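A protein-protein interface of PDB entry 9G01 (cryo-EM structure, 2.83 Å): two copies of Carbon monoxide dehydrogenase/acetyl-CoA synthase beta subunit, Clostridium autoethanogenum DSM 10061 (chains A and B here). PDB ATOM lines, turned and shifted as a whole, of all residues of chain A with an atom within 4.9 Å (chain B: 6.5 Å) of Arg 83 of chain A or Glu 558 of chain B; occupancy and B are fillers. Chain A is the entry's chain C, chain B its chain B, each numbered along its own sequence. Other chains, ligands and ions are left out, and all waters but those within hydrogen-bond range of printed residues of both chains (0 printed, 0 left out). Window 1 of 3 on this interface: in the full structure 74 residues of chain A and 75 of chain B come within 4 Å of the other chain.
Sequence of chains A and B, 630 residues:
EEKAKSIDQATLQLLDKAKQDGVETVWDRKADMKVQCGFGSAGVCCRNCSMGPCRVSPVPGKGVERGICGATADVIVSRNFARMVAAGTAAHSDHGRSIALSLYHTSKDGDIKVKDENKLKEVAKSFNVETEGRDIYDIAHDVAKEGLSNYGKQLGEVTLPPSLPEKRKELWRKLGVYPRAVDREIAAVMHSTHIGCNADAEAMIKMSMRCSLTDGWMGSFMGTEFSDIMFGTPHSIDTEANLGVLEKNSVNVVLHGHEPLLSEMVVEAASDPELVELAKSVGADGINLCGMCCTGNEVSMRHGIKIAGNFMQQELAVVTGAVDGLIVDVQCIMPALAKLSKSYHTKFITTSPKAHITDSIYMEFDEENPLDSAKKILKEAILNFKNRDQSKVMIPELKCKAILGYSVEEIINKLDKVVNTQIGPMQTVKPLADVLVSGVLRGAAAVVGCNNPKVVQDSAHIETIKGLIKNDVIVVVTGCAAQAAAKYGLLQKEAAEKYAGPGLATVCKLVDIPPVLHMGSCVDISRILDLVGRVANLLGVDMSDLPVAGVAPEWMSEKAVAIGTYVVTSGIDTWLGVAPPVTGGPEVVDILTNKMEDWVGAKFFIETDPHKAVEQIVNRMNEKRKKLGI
The guanidinium group (NH1) of Arg 83 of chain B lies within salt-bridge range of the side-chain carboxylate (OE2) of Glu 558 of chain A (2.8 Å). OE2 of Glu 558 of chain B is in salt-bridge range of NH1 of Arg 83 of chain A, at 2.8 Å. NE2 of His 194 of chain A lies within hydrogen-bond range of N of Lys 559 of chain B (3.4 Å). The backbone carbonyl oxygen (O) of Asn 48 of chain A sits close to the side-chain carboxylate (OE2) of Glu 558 of chain B (3.3 Å). The side-chain sulfur of Met 190 of chain B lies close to the side-chain sulfur of Met 190 of chain A (3.7 Å).
The side-chain hydroxyl (OG) of Ser 557 of chain B lies within hydrogen-bond range of the backbone NH (N) of Ala 560 of chain B (3.1 Å). ND2 of Asn 48 of chain A is in hydrogen-bond range of O of Thr 193 of chain A. The guanidinium group of Arg 83 of chain A lies within hydrogen-bond range of the side-chain hydroxyl of Thr 193 of chain A (2.7 Å). The backbone carbonyl oxygen (O) of Met 190 of chain A lies within hydrogen-bond range of the side-chain hydroxyl (OG1) of Thr 193 of chain A, at 3.1 Å.
Arg 83 of chain A touches Ala 87 of chain B. Arg 83 of chain B touches Ala 87 of chain A (NH2 to CB, 3.4 Å). CB of Ala 87 of chain A touches CE of Met 190 of chain B (3.8 Å). Met 190 of chain A touches Ala 87 of chain B. His 194 of chain A touches Ser 557 of chain B. Glu 558 of chain B touches His 194 of chain A (N to NE2, 3.6 Å). Ile 195 of chain A touches Met 556 of chain B.
Of chain B, only Ala 87 and Glu 558 come within 4 Å of Arg 83 of chain A. Glu 558 of chain B touches just these residues of chain A: Asn 48, Arg 83 and His 194. Of the printed residues of chain A, Lys 559 of chain B touches His 194 (3.4 Å). Printed residues of chain B within 4 Å of Ile 195 of chain A: Met 556 (3.8 Å). Val 189 of chain A touches none of the printed residues of chain B. Trp 555 of chain B touches none of the printed residues of chain A. The nearest residue of chain A that does not touch Glu 558 of chain B is Ile 195 of chain A (4.6 Å).
Along chain B the printed residues that touch a printed residue of chain A span positions 83 to 559. Hydrophobic or aromatic side chains of chain A that line the printed part of chain B: Ala 87, Met 190, His 194 and Ile 195. Among the printed residues, Asp or Glu carboxylates within 4 Å of a Lys or Arg side-chain nitrogen of the other chain: Arg 83 of chain A with Glu 558 of chain B (2.8 Å) and Glu 558 of chain A with Arg 83 of chain B (2.8 Å).
Arg 83 of chain A touches Ala 87 of chain B, and with the chains exchanged Ala 87 of chain A touches Arg 83 of chain B. Arg 83 of chain A touches Glu 558 of chain B, and with the chains exchanged Glu 558 of chain A touches Arg 83 of chain B. Ala 87 of chain A touches Met 190 of chain B, and with the chains exchanged Met 190 of chain A touches Ala 87 of chain B. Met 190 of chain A touches its own counterpart, Met 190 of chain B.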
ATOM      1  N   ASN A  48      15.296   1.376  13.353  1.00  0.00           N
ATOM      2  CA  ASN A  48      13.853   1.467  13.518  1.00  0.00           C
ATOM      3  C   ASN A  48      13.086   1.612  12.206  1.00  0.00           C
ATOM      4  O   ASN A  48      11.869   1.431  12.216  1.00  0.00           O
ATOM      5  CB  ASN A  48      13.517   2.625  14.466  1.00  0.00           C
ATOM      6  CG  ASN A  48      13.875   2.307  15.923  1.00  0.00           C
ATOM      7  OD1 ASN A  48      14.613   1.362  16.170  1.00  0.00           O
ATOM      8  ND2 ASN A  48      13.358   3.083  16.879  1.00  0.00           N
ATOM      9  N   ARG A  79      15.485   6.274  22.370  1.00  0.00           N
ATOM     10  CA  ARG A  79      14.544   5.297  21.819  1.00  0.00           C
ATOM     11  C   ARG A  79      15.006   3.865  22.084  1.00  0.00           C
ATOM     12  O   ARG A  79      14.203   3.019  22.499  1.00  0.00           O
ATOM     13  CB  ARG A  79      14.324   5.549  20.323  1.00  0.00           C
ATOM     14  CG  ARG A  79      13.600   6.902  20.044  1.00  0.00           C
ATOM     15  CD  ARG A  79      13.154   7.054  18.572  1.00  0.00           C
ATOM     16  NE  ARG A  79      14.257   6.894  17.629  1.00  0.00           N
ATOM     17  CZ  ARG A  79      14.182   7.180  16.336  1.00  0.00           C
ATOM     18  NH1 ARG A  79      13.095   7.715  15.812  1.00  0.00           N
ATOM     19  NH2 ARG A  79      15.226   6.914  15.544  1.00  0.00           N
ATOM     20  N   ASN A  80      16.304   3.587  21.914  1.00  0.00           N
ATOM     21  CA  ASN A  80      16.816   2.247  22.212  1.00  0.00           C
ATOM     22  C   ASN A  80      16.586   1.888  23.677  1.00  0.00           C
ATOM     23  O   ASN A  80      16.122   0.779  24.000  1.00  0.00           O
ATOM     24  CB  ASN A  80      18.311   2.170  21.874  1.00  0.00           C
ATOM     25  CG  ASN A  80      18.591   2.199  20.360  1.00  0.00           C
ATOM     26  OD1 ASN A  80      17.725   1.857  19.567  1.00  0.00           O
ATOM     27  ND2 ASN A  80      19.800   2.601  19.969  1.00  0.00           N
ATOM     28  N   PHE A  81      16.869   2.825  24.577  1.00  0.00           N
ATOM     29  CA  PHE A  81      16.641   2.580  25.999  1.00  0.00           C
ATOM     30  C   PHE A  81      15.164   2.319  26.293  1.00  0.00           C
ATOM     31  O   PHE A  81      14.816   1.368  27.010  1.00  0.00           O
ATOM     32  CB  PHE A  81      17.152   3.770  26.816  1.00  0.00           C
ATOM     33  CG  PHE A  81      17.006   3.588  28.306  1.00  0.00           C
ATOM     34  CD1 PHE A  81      18.021   2.966  29.042  1.00  0.00           C
ATOM     35  CD2 PHE A  81      15.850   4.021  28.974  1.00  0.00           C
ATOM     36  CE1 PHE A  81      17.898   2.772  30.434  1.00  0.00           C
ATOM     37  CE2 PHE A  81      15.711   3.836  30.373  1.00  0.00           C
ATOM     38  CZ  PHE A  81      16.744   3.209  31.100  1.00  0.00           C
ATOM     39  N   ALA A  82      14.279   3.118  25.694  1.00  0.00           N
ATOM     40  CA  ALA A  82      12.843   2.958  25.904  1.00  0.00           C
ATOM     41  C   ALA A  82      12.358   1.597  25.427  1.00  0.00           C
ATOM     42  O   ALA A  82      11.532   0.959  26.090  1.00  0.00           O
ATOM     43  CB  ALA A  82      12.077   4.080  25.202  1.00  0.00           C
ATOM     44  N   ARG A  83      12.883   1.117  24.303  1.00  0.00           N
ATOM     45  CA  ARG A  83      12.476  -0.195  23.799  1.00  0.00           C
ATOM     46  C   ARG A  83      12.977  -1.307  24.718  1.00  0.00           C
ATOM     47  O   ARG A  83      12.277  -2.309  24.921  1.00  0.00           O
ATOM     48  CB  ARG A  83      12.956  -0.386  22.352  1.00  0.00           C
ATOM     49  CG  ARG A  83      12.135   0.464  21.332  1.00  0.00           C
ATOM     50  CD  ARG A  83      12.048  -0.172  19.911  1.00  0.00           C
ATOM     51  NE  ARG A  83      11.121   0.579  19.076  1.00  0.00           N
ATOM     52  CZ  ARG A  83      10.915   0.422  17.776  1.00  0.00           C
ATOM     53  NH1 ARG A  83      11.595  -0.455  17.068  1.00  0.00           N
ATOM     54  NH2 ARG A  83       9.996   1.179  17.169  1.00  0.00           N
ATOM     55  N   MET A  84      14.163  -1.149  25.306  1.00  0.00           N
ATOM     56  CA  MET A  84      14.591  -2.135  26.302  1.00  0.00           C
ATOM     57  C   MET A  84      13.623  -2.170  27.480  1.00  0.00           C
ATOM     58  O   MET A  84      13.233  -3.253  27.951  1.00  0.00           O
ATOM     59  CB  MET A  84      15.997  -1.822  26.808  1.00  0.00           C
ATOM     60  CG  MET A  84      17.044  -1.872  25.715  1.00  0.00           C
ATOM     61  SD  MET A  84      18.704  -1.724  26.401  1.00  0.00           S
ATOM     62  CE  MET A  84      18.949  -3.345  27.110  1.00  0.00           C
ATOM     63  N   VAL A  85      13.217  -0.995  27.963  1.00  0.00           N
ATOM     64  CA  VAL A  85      12.259  -0.940  29.068  1.00  0.00           C
ATOM     65  C   VAL A  85      10.939  -1.598  28.669  1.00  0.00           C
ATOM     66  O   VAL A  85      10.344  -2.350  29.451  1.00  0.00           O
ATOM     67  CB  VAL A  85      12.049   0.517  29.529  1.00  0.00           C
ATOM     68  CG1 VAL A  85      10.821   0.626  30.437  1.00  0.00           C
ATOM     69  CG2 VAL A  85      13.315   1.071  30.243  1.00  0.00           C
ATOM     70  N   ALA A  86      10.459  -1.325  27.453  1.00  0.00           N
ATOM     71  CA  ALA A  86       9.193  -1.900  26.999  1.00  0.00           C
ATOM     72  C   ALA A  86       9.277  -3.416  26.917  1.00  0.00           C
ATOM     73  O   ALA A  86       8.337  -4.118  27.303  1.00  0.00           O
ATOM     74  CB  ALA A  86       8.793  -1.310  25.642  1.00  0.00           C
ATOM     75  N   ALA A  87      10.399  -3.946  26.433  1.00  0.00           N
ATOM     76  CA  ALA A  87      10.554  -5.397  26.362  1.00  0.00           C
ATOM     77  C   ALA A  87      10.569  -6.032  27.755  1.00  0.00           C
ATOM     78  O   ALA A  87       9.895  -7.047  27.993  1.00  0.00           O
ATOM     79  CB  ALA A  87      11.834  -5.737  25.591  1.00  0.00           C
ATOM     80  N   VAL A 189       4.919   3.137  24.385  1.00  0.00           N
ATOM     81  CA  VAL A 189       6.365   3.227  24.190  1.00  0.00           C
ATOM     82  C   VAL A 189       6.738   2.761  22.786  1.00  0.00           C
ATOM     83  O   VAL A 189       7.503   3.425  22.078  1.00  0.00           O
ATOM     84  CB  VAL A 189       7.117   2.425  25.267  1.00  0.00           C
ATOM     85  CG1 VAL A 189       8.598   2.260  24.857  1.00  0.00           C
ATOM     86  CG2 VAL A 189       6.972   3.096  26.655  1.00  0.00           C
ATOM     87  N   MET A 190       6.167   1.637  22.340  1.00  0.00           N
ATOM     88  CA  MET A 190       6.477   1.167  20.987  1.00  0.00           C
ATOM     89  C   MET A 190       6.016   2.166  19.930  1.00  0.00           C
ATOM     90  O   MET A 190       6.690   2.340  18.906  1.00  0.00           O
ATOM     91  CB  MET A 190       5.832  -0.206  20.735  1.00  0.00           C
ATOM     92  CG  MET A 190       6.423  -1.358  21.591  1.00  0.00           C
ATOM     93  SD  MET A 190       8.201  -1.589  21.320  1.00  0.00           S
ATOM     94  CE  MET A 190       8.278  -2.118  19.605  1.00  0.00           C
ATOM     95  N   THR A 193       8.536   5.366  19.728  1.00  0.00           N
ATOM     96  CA  THR A 193       9.844   5.104  19.136  1.00  0.00           C
ATOM     97  C   THR A 193       9.790   4.873  17.624  1.00  0.00           C
ATOM     98  O   THR A 193      10.846   4.805  16.987  1.00  0.00           O
ATOM     99  CB  THR A 193      10.516   3.899  19.817  1.00  0.00           C
ATOM    100  OG1 THR A 193       9.655   2.761  19.732  1.00  0.00           O
ATOM    101  CG2 THR A 193      10.830   4.209  21.297  1.00  0.00           C
ATOM    102  N   HIS A 194       8.597   4.761  17.037  1.00  0.00           N
ATOM    103  CA  HIS A 194       8.468   4.618  15.590  1.00  0.00           C
ATOM    104  C   HIS A 194       9.078   5.817  14.862  1.00  0.00           C
ATOM    105  O   HIS A 194       9.087   6.939  15.377  1.00  0.00           O
ATOM    106  CB  HIS A 194       6.980   4.475  15.235  1.00  0.00           C
ATOM    107  CG  HIS A 194       6.712   4.205  13.785  1.00  0.00           C
ATOM    108  ND1 HIS A 194       6.756   5.181  12.823  1.00  0.00           N
ATOM    109  CD2 HIS A 194       6.381   3.061  13.139  1.00  0.00           C
ATOM    110  CE1 HIS A 194       6.479   4.659  11.645  1.00  0.00           C
ATOM    111  NE2 HIS A 194       6.243   3.366  11.810  1.00  0.00           N
ATOM    112  N   ILE A 195       9.587   5.573  13.643  1.00  0.00           N
ATOM    113  CA  ILE A 195      10.267   6.624  12.887  1.00  0.00           C
ATOM    114  C   ILE A 195       9.372   7.846  12.824  1.00  0.00           C
ATOM    115  O   ILE A 195       8.158   7.733  12.609  1.00  0.00           O
ATOM    116  CB  ILE A 195      10.661   6.116  11.479  1.00  0.00           C
ATOM    117  CG1 ILE A 195      11.112   7.249  10.544  1.00  0.00           C
ATOM    118  CG2 ILE A 195       9.488   5.454  10.744  1.00  0.00           C
ATOM    119  CD1 ILE A 195      12.327   7.962  10.955  1.00  0.00           C
ATOM    120  N   GLU A 558      16.674  -7.343  29.439  1.00  0.00           N
ATOM    121  CA  GLU A 558      15.784  -6.189  29.342  1.00  0.00           C
ATOM    122  C   GLU A 558      14.913  -6.070  30.585  1.00  0.00           C
ATOM    123  O   GLU A 558      14.605  -4.954  31.027  1.00  0.00           O
ATOM    124  CB  GLU A 558      14.927  -6.298  28.070  1.00  0.00           C
ATOM    125  CG  GLU A 558      15.742  -6.053  26.775  1.00  0.00           C
ATOM    126  CD  GLU A 558      15.039  -6.546  25.501  1.00  0.00           C
ATOM    127  OE1 GLU A 558      14.432  -7.635  25.519  1.00  0.00           O
ATOM    128  OE2 GLU A 558      15.089  -5.833  24.480  1.00  0.00           O
ATOM    129  N   ARG B  83       9.758  -7.684  15.945  1.00  0.00           N
ATOM    130  CA  ARG B  83       9.730  -6.393  16.631  1.00  0.00           C
ATOM    131  C   ARG B  83       9.332  -5.275  15.671  1.00  0.00           C
ATOM    132  O   ARG B  83       8.628  -4.338  16.067  1.00  0.00           O
ATOM    133  CB  ARG B  83      11.082  -6.111  17.304  1.00  0.00           C
ATOM    134  CG  ARG B  83      11.306  -6.977  18.578  1.00  0.00           C
ATOM    135  CD  ARG B  83      12.197  -6.289  19.652  1.00  0.00           C
ATOM    136  NE  ARG B  83      12.215  -7.082  20.874  1.00  0.00           N
ATOM    137  CZ  ARG B  83      13.011  -6.919  21.919  1.00  0.00           C
ATOM    138  NH1 ARG B  83      13.947  -5.994  21.936  1.00  0.00           N
ATOM    139  NH2 ARG B  83      12.865  -7.721  22.977  1.00  0.00           N
ATOM    140  N   MET B  84       9.753  -5.355  14.407  1.00  0.00           N
ATOM    141  CA  MET B  84       9.259  -4.372  13.435  1.00  0.00           C
ATOM    142  C   MET B  84       7.741  -4.450  13.303  1.00  0.00           C
ATOM    143  O   MET B  84       7.051  -3.416  13.291  1.00  0.00           O
ATOM    144  CB  MET B  84       9.899  -4.591  12.067  1.00  0.00           C
ATOM    145  CG  MET B  84      11.403  -4.430  12.080  1.00  0.00           C
ATOM    146  SD  MET B  84      12.072  -4.460  10.407  1.00  0.00           S
ATOM    147  CE  MET B  84      11.593  -2.849   9.800  1.00  0.00           C
ATOM    148  N   VAL B  85       7.206  -5.669  13.212  1.00  0.00           N
ATOM    149  CA  VAL B  85       5.754  -5.837  13.120  1.00  0.00           C
ATOM    150  C   VAL B  85       5.069  -5.271  14.361  1.00  0.00           C
ATOM    151  O   VAL B  85       4.039  -4.591  14.264  1.00  0.00           O
ATOM    152  CB  VAL B  85       5.395  -7.321  12.899  1.00  0.00           C
ATOM    153  CG1 VAL B  85       3.904  -7.561  13.158  1.00  0.00           C
ATOM    154  CG2 VAL B  85       5.787  -7.792  11.470  1.00  0.00           C
ATOM    155  N   ALA B  86       5.622  -5.544  15.544  1.00  0.00           N
ATOM    156  CA  ALA B  86       5.021  -5.059  16.786  1.00  0.00           C
ATOM    157  C   ALA B  86       5.024  -3.538  16.839  1.00  0.00           C
ATOM    158  O   ALA B  86       4.042  -2.925  17.269  1.00  0.00           O
ATOM    159  CB  ALA B  86       5.756  -5.644  17.997  1.00  0.00           C
ATOM    160  N   ALA B  87       6.109  -2.908  16.392  1.00  0.00           N
ATOM    161  CA  ALA B  87       6.156  -1.447  16.382  1.00  0.00           C
ATOM    162  C   ALA B  87       5.120  -0.856  15.422  1.00  0.00           C
ATOM    163  O   ALA B  87       4.406   0.096  15.773  1.00  0.00           O
ATOM    164  CB  ALA B  87       7.568  -0.983  16.013  1.00  0.00           C
ATOM    165  N   GLY B  88       5.008  -1.419  14.212  1.00  0.00           N
ATOM    166  CA  GLY B  88       3.998  -0.940  13.272  1.00  0.00           C
ATOM    167  C   GLY B  88       2.585  -1.114  13.799  1.00  0.00           C
ATOM    168  O   GLY B  88       1.748  -0.201  13.710  1.00  0.00           O
ATOM    169  N   THR B  89       2.316  -2.275  14.402  1.00  0.00           N
ATOM    170  CA  THR B  89       1.017  -2.519  15.010  1.00  0.00           C
ATOM    171  C   THR B  89       0.750  -1.516  16.121  1.00  0.00           C
ATOM    172  O   THR B  89      -0.362  -1.000  16.237  1.00  0.00           O
ATOM    173  CB  THR B  89       0.944  -3.958  15.550  1.00  0.00           C
ATOM    174  OG1 THR B  89       1.190  -4.902  14.499  1.00  0.00           O
ATOM    175  CG2 THR B  89      -0.429  -4.253  16.148  1.00  0.00           C
ATOM    176  N   MET B 190       6.598  -8.682  22.116  1.00  0.00           N
ATOM    177  CA  MET B 190       7.733  -8.125  22.855  1.00  0.00           C
ATOM    178  C   MET B 190       8.247  -9.115  23.896  1.00  0.00           C
ATOM    179  O   MET B 190       9.464  -9.236  24.102  1.00  0.00           O
ATOM    180  CB  MET B 190       7.335  -6.801  23.523  1.00  0.00           C
ATOM    181  CG  MET B 190       7.052  -5.644  22.527  1.00  0.00           C
ATOM    182  SD  MET B 190       8.487  -5.255  21.490  1.00  0.00           S
ATOM    183  CE  MET B 190       9.683  -4.647  22.683  1.00  0.00           C
ATOM    184  N   TRP B 555       8.552   1.295   0.442  1.00  0.00           N
ATOM    185  CA  TRP B 555       8.228   1.381   1.866  1.00  0.00           C
ATOM    186  C   TRP B 555       9.471   1.641   2.722  1.00  0.00           C
ATOM    187  O   TRP B 555      10.593   1.273   2.358  1.00  0.00           O
ATOM    188  CB  TRP B 555       7.538   0.101   2.341  1.00  0.00           C
ATOM    189  CG  TRP B 555       8.491  -1.062   2.416  1.00  0.00           C
ATOM    190  CD1 TRP B 555       8.834  -1.916   1.403  1.00  0.00           C
ATOM    191  CD2 TRP B 555       9.252  -1.480   3.565  1.00  0.00           C
ATOM    192  NE1 TRP B 555       9.755  -2.843   1.849  1.00  0.00           N
ATOM    193  CE2 TRP B 555      10.027  -2.593   3.179  1.00  0.00           C
ATOM    194  CE3 TRP B 555       9.340  -1.006   4.891  1.00  0.00           C
ATOM    195  CZ2 TRP B 555      10.893  -3.266   4.069  1.00  0.00           C
ATOM    196  CZ3 TRP B 555      10.207  -1.675   5.791  1.00  0.00           C
ATOM    197  CH2 TRP B 555      10.968  -2.796   5.366  1.00  0.00           C
ATOM    198  N   MET B 556       9.263   2.304   3.866  1.00  0.00           N
ATOM    199  CA  MET B 556      10.338   2.559   4.823  1.00  0.00           C
ATOM    200  C   MET B 556       9.971   2.235   6.277  1.00  0.00           C
ATOM    201  O   MET B 556      10.851   1.867   7.059  1.00  0.00           O
ATOM    202  CB  MET B 556      10.813   4.022   4.705  1.00  0.00           C
ATOM    203  CG  MET B 556       9.810   5.083   5.216  1.00  0.00           C
ATOM    204  SD  MET B 556       9.906   5.492   6.979  1.00  0.00           S
ATOM    205  CE  MET B 556       8.510   6.606   7.163  1.00  0.00           C
ATOM    206  N   SER B 557       8.698   2.355   6.655  1.00  0.00           N
ATOM    207  CA  SER B 557       8.289   2.386   8.053  1.00  0.00           C
ATOM    208  C   SER B 557       8.002   0.988   8.602  1.00  0.00           C
ATOM    209  O   SER B 557       7.706   0.044   7.866  1.00  0.00           O
ATOM    210  CB  SER B 557       7.055   3.282   8.259  1.00  0.00           C
ATOM    211  OG  SER B 557       5.900   2.769   7.601  1.00  0.00           O
ATOM    212  N   GLU B 558       8.061   0.881   9.930  1.00  0.00           N
ATOM    213  CA  GLU B 558       7.610  -0.337  10.598  1.00  0.00           C
ATOM    214  C   GLU B 558       6.125  -0.569  10.350  1.00  0.00           C
ATOM    215  O   GLU B 558       5.684  -1.721  10.225  1.00  0.00           O
ATOM    216  CB  GLU B 558       7.920  -0.256  12.102  1.00  0.00           C
ATOM    217  CG  GLU B 558       9.430  -0.441  12.411  1.00  0.00           C
ATOM    218  CD  GLU B 558       9.828   0.017  13.822  1.00  0.00           C
ATOM    219  OE1 GLU B 558       9.300   1.039  14.303  1.00  0.00           O
ATOM    220  OE2 GLU B 558      10.667  -0.657  14.454  1.00  0.00           O
ATOM    221  N   LYS B 559       5.349   0.508  10.227  1.00  0.00           N
ATOM    222  CA  LYS B 559       3.946   0.360   9.859  1.00  0.00           C
ATOM    223  C   LYS B 559       3.783  -0.377   8.535  1.00  0.00           C
ATOM    224  O   LYS B 559       2.933  -1.264   8.418  1.00  0.00           O
ATOM    225  CB  LYS B 559       3.279   1.732   9.771  1.00  0.00           C
ATOM    226  CG  LYS B 559       2.862   2.315  11.126  1.00  0.00           C
ATOM    227  CD  LYS B 559       2.177   3.693  10.953  1.00  0.00           C
ATOM    228  CE  LYS B 559       3.187   4.765  10.454  1.00  0.00           C
ATOM    229  NZ  LYS B 559       2.545   6.096  10.121  1.00  0.00           N
ATOM    230  N   ALA B 560       4.647  -0.095   7.560  1.00  0.00           N
ATOM    231  CA  ALA B 560       4.586  -0.803   6.282  1.00  0.00           C
ATOM    232  C   ALA B 560       4.848  -2.292   6.459  1.00  0.00           C
ATOM    233  O   ALA B 560       4.197  -3.125   5.815  1.00  0.00           O
ATOM    234  CB  ALA B 560       5.577  -0.187   5.294  1.00  0.00           C
ATOM    235  N   VAL B 561       5.779  -2.651   7.343  1.00  0.00           N
ATOM    236  CA  VAL B 561       6.053  -4.061   7.609  1.00  0.00           C
ATOM    237  C   VAL B 561       4.818  -4.734   8.189  1.00  0.00           C
ATOM    238  O   VAL B 561       4.391  -5.800   7.726  1.00  0.00           O
ATOM    239  CB  VAL B 561       7.267  -4.217   8.542  1.00  0.00           C
ATOM    240  CG1 VAL B 561       7.484  -5.700   8.877  1.00  0.00           C
ATOM    241  CG2 VAL B 561       8.514  -3.614   7.896  1.00  0.00           C
ATOM    242  N   ALA B 562       4.201  -4.102   9.187  1.00  0.00           N
ATOM    243  CA  ALA B 562       2.993  -4.680   9.779  1.00  0.00           C
ATOM    244  C   ALA B 562       1.878  -4.807   8.744  1.00  0.00           C
ATOM    245  O   ALA B 562       1.151  -5.813   8.721  1.00  0.00           O
ATOM    246  CB  ALA B 562       2.533  -3.836  10.974  1.00  0.00           C
ATOM    247  N   ILE B 563       1.738  -3.810   7.866  1.00  0.00           N
ATOM    248  CA  ILE B 563       0.702  -3.829   6.832  1.00  0.00           C
ATOM    249  C   ILE B 563       0.912  -4.994   5.878  1.00  0.00           C
ATOM    250  O   ILE B 563      -0.010  -5.772   5.611  1.00  0.00           O
ATOM    251  CB  ILE B 563       0.683  -2.494   6.066  1.00  0.00           C
ATOM    252  CG1 ILE B 563       0.081  -1.380   6.922  1.00  0.00           C
ATOM    253  CG2 ILE B 563      -0.101  -2.616   4.725  1.00  0.00           C
ATOM    254  CD1 ILE B 563       0.410   0.003   6.381  1.00  0.00           C
